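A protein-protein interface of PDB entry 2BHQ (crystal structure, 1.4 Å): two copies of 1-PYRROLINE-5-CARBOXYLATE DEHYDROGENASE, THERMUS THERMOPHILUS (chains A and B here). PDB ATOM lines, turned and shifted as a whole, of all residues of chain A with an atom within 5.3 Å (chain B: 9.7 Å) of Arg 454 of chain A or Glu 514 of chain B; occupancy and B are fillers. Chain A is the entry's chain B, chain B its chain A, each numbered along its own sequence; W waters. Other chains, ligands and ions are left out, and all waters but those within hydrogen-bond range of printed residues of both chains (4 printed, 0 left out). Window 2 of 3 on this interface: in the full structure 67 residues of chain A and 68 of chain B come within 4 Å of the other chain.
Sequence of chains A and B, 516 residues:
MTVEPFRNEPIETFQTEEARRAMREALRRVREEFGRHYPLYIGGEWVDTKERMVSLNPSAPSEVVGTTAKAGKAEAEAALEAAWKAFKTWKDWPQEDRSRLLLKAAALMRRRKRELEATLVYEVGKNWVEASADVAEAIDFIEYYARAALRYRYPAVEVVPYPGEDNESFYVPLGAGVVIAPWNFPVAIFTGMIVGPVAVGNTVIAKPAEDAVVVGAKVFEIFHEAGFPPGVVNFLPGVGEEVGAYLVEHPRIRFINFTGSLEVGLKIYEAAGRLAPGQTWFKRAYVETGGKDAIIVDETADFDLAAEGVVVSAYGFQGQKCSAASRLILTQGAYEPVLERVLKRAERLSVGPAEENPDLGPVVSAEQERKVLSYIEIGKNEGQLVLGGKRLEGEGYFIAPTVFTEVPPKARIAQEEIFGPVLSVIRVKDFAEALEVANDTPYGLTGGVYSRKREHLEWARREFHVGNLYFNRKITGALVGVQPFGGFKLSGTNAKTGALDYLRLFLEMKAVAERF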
ATOM      1  N   ARG A 452      -8.970  -9.856  -7.964  1.00  0.00           N
ATOM      2  CA  ARG A 452      -8.570  -9.064  -9.123  1.00  0.00           C
ATOM      3  C   ARG A 452      -8.287  -7.633  -8.665  1.00  0.00           C
ATOM      4  O   ARG A 452      -7.741  -6.827  -9.419  1.00  0.00           O
ATOM      5  CB  ARG A 452      -9.679  -9.009 -10.176  1.00  0.00           C
ATOM      6  CG  ARG A 452      -9.934 -10.285 -10.951  1.00  0.00           C
ATOM      7  CD  ARG A 452     -10.878  -9.964 -12.113  1.00  0.00           C
ATOM      8  NE  ARG A 452     -11.128 -11.092 -13.005  1.00  0.00           N
ATOM      9  CZ  ARG A 452     -12.038 -12.038 -12.797  1.00  0.00           C
ATOM     10  NH1 ARG A 452     -12.183 -13.022 -13.676  1.00  0.00           N
ATOM     11  NH2 ARG A 452     -12.814 -12.000 -11.723  1.00  0.00           N
ATOM     12  N   LYS A 453      -8.663  -7.309  -7.431  1.00  0.00           N
ATOM     13  CA  LYS A 453      -8.461  -5.955  -6.928  1.00  0.00           C
ATOM     14  C   LYS A 453      -7.014  -5.696  -6.522  1.00  0.00           C
ATOM     15  O   LYS A 453      -6.524  -6.249  -5.537  1.00  0.00           O
ATOM     16  CB  LYS A 453      -9.405  -5.687  -5.754  1.00  0.00           C
ATOM     17  CG  LYS A 453      -9.415  -4.232  -5.314  1.00  0.00           C
ATOM     18  CD  LYS A 453     -10.561  -3.933  -4.369  1.00  0.00           C
ATOM     19  CE  LYS A 453     -10.493  -2.495  -3.882  1.00  0.00           C
ATOM     20  NZ  LYS A 453     -10.452  -1.532  -5.018  1.00  0.00           N
ATOM     21  N   ARG A 454      -6.337  -4.842  -7.286  1.00  0.00           N
ATOM     22  CA  ARG A 454      -4.933  -4.529  -7.033  1.00  0.00           C
ATOM     23  C   ARG A 454      -4.671  -4.082  -5.600  1.00  0.00           C
ATOM     24  O   ARG A 454      -3.686  -4.495  -4.985  1.00  0.00           O
ATOM     25  CB  ARG A 454      -4.443  -3.431  -7.983  1.00  0.00           C
ATOM     26  CG  ARG A 454      -4.688  -3.696  -9.466  1.00  0.00           C
ATOM     27  CD  ARG A 454      -4.209  -5.077  -9.914  1.00  0.00           C
ATOM     28  NE  ARG A 454      -2.802  -5.332  -9.602  1.00  0.00           N
ATOM     29  CZ  ARG A 454      -2.205  -6.509  -9.778  1.00  0.00           C
ATOM     30  NH1 ARG A 454      -0.923  -6.659  -9.471  1.00  0.00           N
ATOM     31  NH2 ARG A 454      -2.888  -7.537 -10.263  1.00  0.00           N
ATOM     32  N   GLU A 455      -5.552  -3.237  -5.078  1.00  0.00           N
ATOM     33  CA  GLU A 455      -5.401  -2.716  -3.726  1.00  0.00           C
ATOM     34  C   GLU A 455      -5.420  -3.815  -2.665  1.00  0.00           C
ATOM     35  O   GLU A 455      -4.727  -3.717  -1.655  1.00  0.00           O
ATOM     36  CB  GLU A 455      -6.487  -1.671  -3.435  1.00  0.00           C
ATOM     37  CG  GLU A 455      -6.371  -0.390  -4.274  1.00  0.00           C
ATOM     38  CD  GLU A 455      -6.936  -0.526  -5.684  1.00  0.00           C
ATOM     39  OE1 GLU A 455      -7.398  -1.624  -6.050  1.00  0.00           O
ATOM     40  OE2 GLU A 455      -6.919   0.481  -6.429  1.00  0.00           O
ATOM     41  N   HIS A 456      -6.213  -4.858  -2.891  1.00  0.00           N
ATOM     42  CA  HIS A 456      -6.275  -5.965  -1.942  1.00  0.00           C
ATOM     43  C   HIS A 456      -4.997  -6.797  -2.019  1.00  0.00           C
ATOM     44  O   HIS A 456      -4.446  -7.197  -0.997  1.00  0.00           O
ATOM     45  CB  HIS A 456      -7.494  -6.846  -2.220  1.00  0.00           C
ATOM     46  CG  HIS A 456      -8.793  -6.224  -1.810  1.00  0.00           C
ATOM     47  ND1 HIS A 456     -10.000  -6.879  -1.923  1.00  0.00           N
ATOM     48  CD2 HIS A 456      -9.071  -5.014  -1.265  1.00  0.00           C
ATOM     49  CE1 HIS A 456     -10.966  -6.101  -1.465  1.00  0.00           C
ATOM     50  NE2 HIS A 456     -10.430  -4.965  -1.059  1.00  0.00           N
ATOM     51  N   LEU A 457      -4.529  -7.057  -3.236  1.00  0.00           N
ATOM     52  CA  LEU A 457      -3.305  -7.826  -3.415  1.00  0.00           C
ATOM     53  C   LEU A 457      -2.105  -7.111  -2.797  1.00  0.00           C
ATOM     54  O   LEU A 457      -1.341  -7.713  -2.045  1.00  0.00           O
ATOM     55  CB  LEU A 457      -3.050  -8.075  -4.904  1.00  0.00           C
ATOM     56  CG  LEU A 457      -4.071  -8.957  -5.632  1.00  0.00           C
ATOM     57  CD1 LEU A 457      -3.628  -9.145  -7.079  1.00  0.00           C
ATOM     58  CD2 LEU A 457      -4.189 -10.312  -4.935  1.00  0.00           C
ATOM     59  N   GLU A 458      -1.933  -5.826  -3.097  1.00  0.00           N
ATOM     60  CA  GLU A 458      -0.787  -5.109  -2.544  1.00  0.00           C
ATOM     61  C   GLU A 458      -0.919  -4.942  -1.027  1.00  0.00           C
ATOM     62  O   GLU A 458       0.078  -4.890  -0.307  1.00  0.00           O
ATOM     63  CB  GLU A 458      -0.603  -3.761  -3.253  1.00  0.00           C
ATOM     64  CG  GLU A 458      -0.387  -3.886  -4.772  1.00  0.00           C
ATOM     65  CD  GLU A 458       0.817  -4.748  -5.164  1.00  0.00           C
ATOM     66  OE1 GLU A 458       0.975  -5.039  -6.376  1.00  0.00           O
ATOM     67  OE2 GLU A 458       1.607  -5.131  -4.275  1.00  0.00           O
ATOM     68  N   TRP A 459      -2.153  -4.874  -0.543  1.00  0.00           N
ATOM     69  CA  TRP A 459      -2.420  -4.778   0.887  1.00  0.00           C
ATOM     70  C   TRP A 459      -1.897  -6.075   1.528  1.00  0.00           C
ATOM     71  O   TRP A 459      -1.205  -6.055   2.549  1.00  0.00           O
ATOM     72  CB  TRP A 459      -3.930  -4.646   1.088  1.00  0.00           C
ATOM     73  CG  TRP A 459      -4.424  -4.450   2.486  1.00  0.00           C
ATOM     74  CD1 TRP A 459      -3.696  -4.458   3.638  1.00  0.00           C
ATOM     75  CD2 TRP A 459      -5.788  -4.242   2.873  1.00  0.00           C
ATOM     76  NE1 TRP A 459      -4.524  -4.269   4.724  1.00  0.00           N
ATOM     77  CE2 TRP A 459      -5.814  -4.134   4.278  1.00  0.00           C
ATOM     78  CE3 TRP A 459      -6.992  -4.138   2.162  1.00  0.00           C
ATOM     79  CZ2 TRP A 459      -7.002  -3.925   4.994  1.00  0.00           C
ATOM     80  CZ3 TRP A 459      -8.174  -3.930   2.872  1.00  0.00           C
ATOM     81  CH2 TRP A 459      -8.167  -3.825   4.275  1.00  0.00           C
ATOM     82  N   ARG A 461       0.335  -8.087   0.288  1.00  0.00           N
ATOM     83  CA  ARG A 461       1.783  -8.152   0.128  1.00  0.00           C
ATOM     84  C   ARG A 461       2.448  -7.522   1.345  1.00  0.00           C
ATOM     85  O   ARG A 461       3.497  -7.975   1.797  1.00  0.00           O
ATOM     86  CB  ARG A 461       2.215  -7.401  -1.144  1.00  0.00           C
ATOM     87  CG  ARG A 461       3.734  -7.411  -1.410  1.00  0.00           C
ATOM     88  CD  ARG A 461       4.084  -6.667  -2.706  1.00  0.00           C
ATOM     89  NE  ARG A 461       3.411  -7.277  -3.849  1.00  0.00           N
ATOM     90  CZ  ARG A 461       3.904  -8.276  -4.576  1.00  0.00           C
ATOM     91  NH1 ARG A 461       5.104  -8.781  -4.305  1.00  0.00           N
ATOM     92  NH2 ARG A 461       3.170  -8.811  -5.542  1.00  0.00           N
ATOM     93  N   PHE A 471      -0.373 -15.082  -5.092  1.00  0.00           N
ATOM     94  CA  PHE A 471      -1.588 -14.441  -5.581  1.00  0.00           C
ATOM     95  C   PHE A 471      -2.118 -15.084  -6.855  1.00  0.00           C
ATOM     96  O   PHE A 471      -1.398 -15.204  -7.848  1.00  0.00           O
ATOM     97  CB  PHE A 471      -1.352 -12.949  -5.858  1.00  0.00           C
ATOM     98  CG  PHE A 471      -0.926 -12.155  -4.654  1.00  0.00           C
ATOM     99  CD1 PHE A 471      -1.349 -12.507  -3.376  1.00  0.00           C
ATOM    100  CD2 PHE A 471      -0.130 -11.021  -4.809  1.00  0.00           C
ATOM    101  CE1 PHE A 471      -0.982 -11.742  -2.263  1.00  0.00           C
ATOM    102  CE2 PHE A 471       0.240 -10.249  -3.704  1.00  0.00           C
ATOM    103  CZ  PHE A 471      -0.190 -10.614  -2.424  1.00  0.00           C
ATOM    104  N   ASN A 472      -3.385 -15.489  -6.806  1.00  0.00           N
ATOM    105  CA  ASN A 472      -4.078 -16.094  -7.931  1.00  0.00           C
ATOM    106  C   ASN A 472      -3.435 -17.358  -8.480  1.00  0.00           C
ATOM    107  O   ASN A 472      -3.396 -17.587  -9.692  1.00  0.00           O
ATOM    108  CB  ASN A 472      -4.289 -15.044  -9.029  1.00  0.00           C
ATOM    109  CG  ASN A 472      -5.236 -13.941  -8.585  1.00  0.00           C
ATOM    110  OD1 ASN A 472      -6.274 -14.217  -7.982  1.00  0.00           O
ATOM    111  ND2 ASN A 472      -4.887 -12.692  -8.873  1.00  0.00           N
ATOM    112  N   TYR B 162      10.339 -16.827 -13.167  1.00  0.00           N
ATOM    113  CA  TYR B 162       9.478 -17.901 -13.636  1.00  0.00           C
ATOM    114  C   TYR B 162       8.478 -17.315 -14.626  1.00  0.00           C
ATOM    115  O   TYR B 162       7.943 -16.226 -14.411  1.00  0.00           O
ATOM    116  CB  TYR B 162       8.730 -18.534 -12.461  1.00  0.00           C
ATOM    117  CG  TYR B 162       8.039 -19.828 -12.818  1.00  0.00           C
ATOM    118  CD1 TYR B 162       8.763 -21.014 -12.938  1.00  0.00           C
ATOM    119  CD2 TYR B 162       6.668 -19.865 -13.067  1.00  0.00           C
ATOM    120  CE1 TYR B 162       8.137 -22.204 -13.297  1.00  0.00           C
ATOM    121  CE2 TYR B 162       6.035 -21.049 -13.427  1.00  0.00           C
ATOM    122  CZ  TYR B 162       6.777 -22.213 -13.538  1.00  0.00           C
ATOM    123  OH  TYR B 162       6.159 -23.395 -13.886  1.00  0.00           O
ATOM    124  N   PRO B 163       8.201 -18.037 -15.717  1.00  0.00           N
ATOM    125  CA  PRO B 163       7.258 -17.575 -16.744  1.00  0.00           C
ATOM    126  C   PRO B 163       5.859 -17.214 -16.238  1.00  0.00           C
ATOM    127  O   PRO B 163       5.259 -17.955 -15.456  1.00  0.00           O
ATOM    128  CB  PRO B 163       7.215 -18.750 -17.722  1.00  0.00           C
ATOM    129  CG  PRO B 163       8.573 -19.372 -17.575  1.00  0.00           C
ATOM    130  CD  PRO B 163       8.779 -19.342 -16.082  1.00  0.00           C
ATOM    131  N   GLY B 164       5.358 -16.069 -16.701  1.00  0.00           N
ATOM    132  CA  GLY B 164       4.024 -15.606 -16.348  1.00  0.00           C
ATOM    133  C   GLY B 164       3.791 -15.213 -14.905  1.00  0.00           C
ATOM    134  O   GLY B 164       2.643 -15.088 -14.476  1.00  0.00           O
ATOM    135  N   GLU B 165       4.871 -14.994 -14.163  1.00  0.00           N
ATOM    136  CA  GLU B 165       4.781 -14.640 -12.752  1.00  0.00           C
ATOM    137  C   GLU B 165       5.768 -13.571 -12.341  1.00  0.00           C
ATOM    138  O   GLU B 165       6.832 -13.423 -12.941  1.00  0.00           O
ATOM    139  CB  GLU B 165       5.118 -15.844 -11.870  1.00  0.00           C
ATOM    140  CG  GLU B 165       4.073 -16.912 -11.730  1.00  0.00           C
ATOM    141  CD  GLU B 165       4.465 -17.960 -10.693  1.00  0.00           C
ATOM    142  OE1 GLU B 165       3.601 -18.785 -10.346  1.00  0.00           O
ATOM    143  OE2 GLU B 165       5.631 -17.966 -10.227  1.00  0.00           O
ATOM    144  N   ASP B 166       5.403 -12.837 -11.297  1.00  0.00           N
ATOM    145  CA  ASP B 166       6.309 -11.870 -10.698  1.00  0.00           C
ATOM    146  C   ASP B 166       6.664 -12.556  -9.382  1.00  0.00           C
ATOM    147  O   ASP B 166       5.775 -12.971  -8.641  1.00  0.00           O
ATOM    148  CB  ASP B 166       5.620 -10.537 -10.392  1.00  0.00           C
ATOM    149  CG  ASP B 166       6.566  -9.533  -9.744  1.00  0.00           C
ATOM    150  OD1 ASP B 166       6.360  -9.157  -8.565  1.00  0.00           O
ATOM    151  OD2 ASP B 166       7.529  -9.123 -10.421  1.00  0.00           O
ATOM    152  N   ASN B 167       7.952 -12.716  -9.112  1.00  0.00           N
ATOM    153  CA  ASN B 167       8.404 -13.328  -7.871  1.00  0.00           C
ATOM    154  C   ASN B 167       9.312 -12.321  -7.206  1.00  0.00           C
ATOM    155  O   ASN B 167      10.378 -11.983  -7.717  1.00  0.00           O
ATOM    156  CB  ASN B 167       9.114 -14.644  -8.160  1.00  0.00           C
ATOM    157  CG  ASN B 167       8.132 -15.765  -8.405  1.00  0.00           C
ATOM    158  OD1 ASN B 167       7.539 -16.294  -7.465  1.00  0.00           O
ATOM    159  ND2 ASN B 167       7.923 -16.110  -9.671  1.00  0.00           N
ATOM    160  N   GLU B 168       8.859 -11.837  -6.060  1.00  0.00           N
ATOM    161  CA  GLU B 168       9.562 -10.797  -5.332  1.00  0.00           C
ATOM    162  C   GLU B 168       9.847 -11.174  -3.892  1.00  0.00           C
ATOM    163  O   GLU B 168       8.927 -11.424  -3.113  1.00  0.00           O
ATOM    164  CB  GLU B 168       8.696  -9.540  -5.370  1.00  0.00           C
ATOM    165  CG  GLU B 168       9.306  -8.292  -4.788  1.00  0.00           C
ATOM    166  CD  GLU B 168       8.327  -7.140  -4.845  1.00  0.00           C
ATOM    167  OE1 GLU B 168       7.450  -7.054  -3.956  1.00  0.00           O
ATOM    168  OE2 GLU B 168       8.414  -6.338  -5.796  1.00  0.00           O
ATOM    169  N   SER B 169      11.125 -11.218  -3.538  1.00  0.00           N
ATOM    170  CA  SER B 169      11.509 -11.525  -2.174  1.00  0.00           C
ATOM    171  C   SER B 169      12.130 -10.270  -1.581  1.00  0.00           C
ATOM    172  O   SER B 169      12.882  -9.554  -2.253  1.00  0.00           O
ATOM    173  CB  SER B 169      12.492 -12.698  -2.139  1.00  0.00           C
ATOM    174  OG  SER B 169      11.789 -13.914  -2.355  1.00  0.00           O
ATOM    175  N   ALA B 511       8.631 -13.948   0.609  1.00  0.00           N
ATOM    176  CA  ALA B 511       8.646 -14.198  -0.829  1.00  0.00           C
ATOM    177  C   ALA B 511       7.211 -14.128  -1.316  1.00  0.00           C
ATOM    178  O   ALA B 511       6.359 -14.887  -0.855  1.00  0.00           O
ATOM    179  CB  ALA B 511       9.241 -15.574  -1.129  1.00  0.00           C
ATOM    180  N   VAL B 512       6.944 -13.219  -2.248  1.00  0.00           N
ATOM    181  CA  VAL B 512       5.596 -13.040  -2.773  1.00  0.00           C
ATOM    182  C   VAL B 512       5.543 -13.256  -4.280  1.00  0.00           C
ATOM    183  O   VAL B 512       6.270 -12.620  -5.045  1.00  0.00           O
ATOM    184  CB  VAL B 512       5.067 -11.629  -2.452  1.00  0.00           C
ATOM    185  CG1 VAL B 512       3.612 -11.505  -2.883  1.00  0.00           C
ATOM    186  CG2 VAL B 512       5.212 -11.352  -0.960  1.00  0.00           C
ATOM    187  N   ALA B 513       4.666 -14.157  -4.697  1.00  0.00           N
ATOM    188  CA  ALA B 513       4.504 -14.482  -6.106  1.00  0.00           C
ATOM    189  C   ALA B 513       3.118 -14.115  -6.620  1.00  0.00           C
ATOM    190  O   ALA B 513       2.117 -14.348  -5.938  1.00  0.00           O
ATOM    191  CB  ALA B 513       4.738 -15.971  -6.309  1.00  0.00           C
ATOM    192  N   GLU B 514       3.058 -13.509  -7.800  1.00  0.00           N
ATOM    193  CA  GLU B 514       1.770 -13.209  -8.411  1.00  0.00           C
ATOM    194  C   GLU B 514       1.740 -13.847  -9.788  1.00  0.00           C
ATOM    195  O   GLU B 514       2.599 -13.571 -10.622  1.00  0.00           O
ATOM    196  CB  GLU B 514       1.489 -11.708  -8.572  1.00  0.00           C
ATOM    197  CG  GLU B 514       0.160 -11.511  -9.323  1.00  0.00           C
ATOM    198  CD  GLU B 514      -0.343 -10.083  -9.410  1.00  0.00           C
ATOM    199  OE1 GLU B 514       0.271  -9.174  -8.821  1.00  0.00           O
ATOM    200  OE2 GLU B 514      -1.381  -9.881 -10.084  1.00  0.00           O
ATOM    201  N   ARG B 515       0.766 -14.721 -10.011  1.00  0.00           N
ATOM    202  CA  ARG B 515       0.603 -15.362 -11.311  1.00  0.00           C
ATOM    203  C   ARG B 515      -0.383 -14.467 -12.057  1.00  0.00           C
ATOM    204  O   ARG B 515      -1.522 -14.296 -11.623  1.00  0.00           O
ATOM    205  CB  ARG B 515       0.023 -16.769 -11.142  1.00  0.00           C
ATOM    206  CG  ARG B 515      -0.220 -17.508 -12.455  1.00  0.00           C
ATOM    207  CD  ARG B 515       1.082 -17.895 -13.127  1.00  0.00           C
ATOM    208  NE  ARG B 515       1.863 -18.835 -12.325  1.00  0.00           N
ATOM    209  CZ  ARG B 515       1.521 -20.100 -12.100  1.00  0.00           C
ATOM    210  NH1 ARG B 515       2.299 -20.876 -11.355  1.00  0.00           N
ATOM    211  NH2 ARG B 515       0.408 -20.592 -12.623  1.00  0.00           N
ATOM    212  N   PHE B 516       0.057 -13.888 -13.167  1.00  0.00           N
ATOM    213  CA  PHE B 516      -0.788 -12.980 -13.934  1.00  0.00           C
ATOM    214  C   PHE B 516      -1.871 -13.646 -14.772  1.00  0.00           C
ATOM    215  O   PHE B 516      -2.900 -12.975 -15.014  1.00  0.00           O
ATOM    216  CB  PHE B 516       0.093 -12.083 -14.805  1.00  0.00           C
ATOM    217  CG  PHE B 516       1.034 -11.231 -14.009  1.00  0.00           C
ATOM    218  CD1 PHE B 516       2.410 -11.424 -14.092  1.00  0.00           C
ATOM    219  CD2 PHE B 516       0.543 -10.257 -13.144  1.00  0.00           C
ATOM    220  CE1 PHE B 516       3.281 -10.657 -13.321  1.00  0.00           C
ATOM    221  CE2 PHE B 516       1.405  -9.487 -12.372  1.00  0.00           C
ATOM    222  CZ  PHE B 516       2.776  -9.687 -12.460  1.00  0.00           C
ATOM    223  OXT PHE B 516      -1.681 -14.808 -15.182  1.00  0.00           O
HETATM  224  O   HOH W   1      -3.393 -16.322 -12.122  1.00  0.00           O
HETATM  225  O   HOH W   2       0.558  -7.961  -6.375  1.00  0.00           O
HETATM  226  O   HOH W   3      -2.825 -12.045 -10.754  1.00  0.00           O
HETATM  227  O   HOH W   4       5.164 -10.522  -6.657  1.00  0.00           O
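OE1 of Glu 168 of chain B lies within salt-bridge range of NH1 of Arg 461 of chain A, at 2.9 Å. N of Phe 471 of chain A sits at hydrogen-bond distance from O of Ala 513 of chain B. NH2 of Arg 454 of chain A is in salt-bridge range of OE2 of Glu 514 of chain B (2.8 Å). The backbone carbonyl oxygen (O) of Phe 471 of chain A lies within hydrogen-bond range of the backbone NH (N) of Arg 515 of chain B, at 3.1 Å.
O of Asp 166 of chain B sits at hydrogen-bond distance from N of Glu 514 of chain B (2.9 Å). NE of Arg 461 of chain A lies within salt-bridge range of OE2 of Glu 458 of chain A, 2.8 Å away. OE1 of Glu 458 of chain A is in salt-bridge range of NH1 of Arg 454 of chain A (3.98 Å). The backbone carbonyl oxygen (O) of Glu 168 of chain B sits at hydrogen-bond distance from the backbone NH (N) of Val 512 of chain B (2.8 Å). NE of Arg 515 of chain B lies within salt-bridge range of OE1 of Glu 165 of chain B, at 2.6 Å.
Among the printed residues, merely in contact across the chains: Arg 461 of chain A with Val 512 of chain B (3.4 Å), Phe 471 of chain A with Val 512 of chain B (3.7 Å), Phe 471 of chain A with Glu 514 of chain B (3.8 Å), Asn 472 of chain A with Arg 515 of chain B (3.8 Å) and Leu 457 of chain A with Glu 514 of chain B (3.8 Å).
Printed residues of chain B within 4 Å of Arg 454 of chain A: Glu 514 (2.8 Å). No residue of chain B comes within 4 Å of Glu 455 of chain A. Glu 458 of chain A touches none of the printed residues of chain B. Of the printed residues of chain A, Glu 168 of chain B touches Arg 461 (2.9 Å). Glu 514 of chain B touches three residues of chain A. Of the printed residues of chain A, Arg 515 of chain B touches Phe 471 and Asn 472. The nearest residue of chain B that does not touch Arg 454 of chain A is Phe 516 of chain B (4.7 Å).
Of the 14 printed residues of chain B, 5 touch a printed residue of chain A. Printed residues of chain B that touch a printed residue of chain A: Glu 168, Val 512, Ala 513, Glu 514 and Arg 515. Hydrophobic or aromatic side chains of chain B that line the printed part of chain A: Val 512. Of the 11 printed residues of chain A, 5 touch a printed residue of chain B. Among the printed residues, Asp or Glu carboxylates within 4 Å of a Lys or Arg side-chain nitrogen of the other chain: Arg 454 of chain A with Glu 514 of chain B (2.8 Å) and Arg 461 of chain A with Glu 168 of chain B (2.9 Å).
No position is printed for both chains. Of the 9 pairs that touch across the chains among the printed residues, none has its exchanged pair printed and touching as well.
Water W4 lies within hydrogen-bond range of the side-chain carboxylate of Asp 166 of chain B (2.6 Å), the guanidinium group of Arg 461 of chain A (2.9 Å) and the backbone carbonyl oxygen of Val 512 of chain B (2.9 Å). Water W3 lies within hydrogen-bond range of OE2 of Glu 514 of chain B (2.7 Å), O of Arg 515 of chain B (2.7 Å) and ND2 of Asn 472 of chain A (2.9 Å). Water W1 bridges O of Asn 472 of chain A (2.7 Å) and O of Arg 515 of chain B (2.8 Å). Water W2 lies within hydrogen-bond range of the side-chain carboxylate of Glu 514 of chain B (2.7 Å), the guanidinium group of Arg 461 of chain A (2.9 Å) and the side-chain carboxylate of Glu 458 of chain A (3.0 Å).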
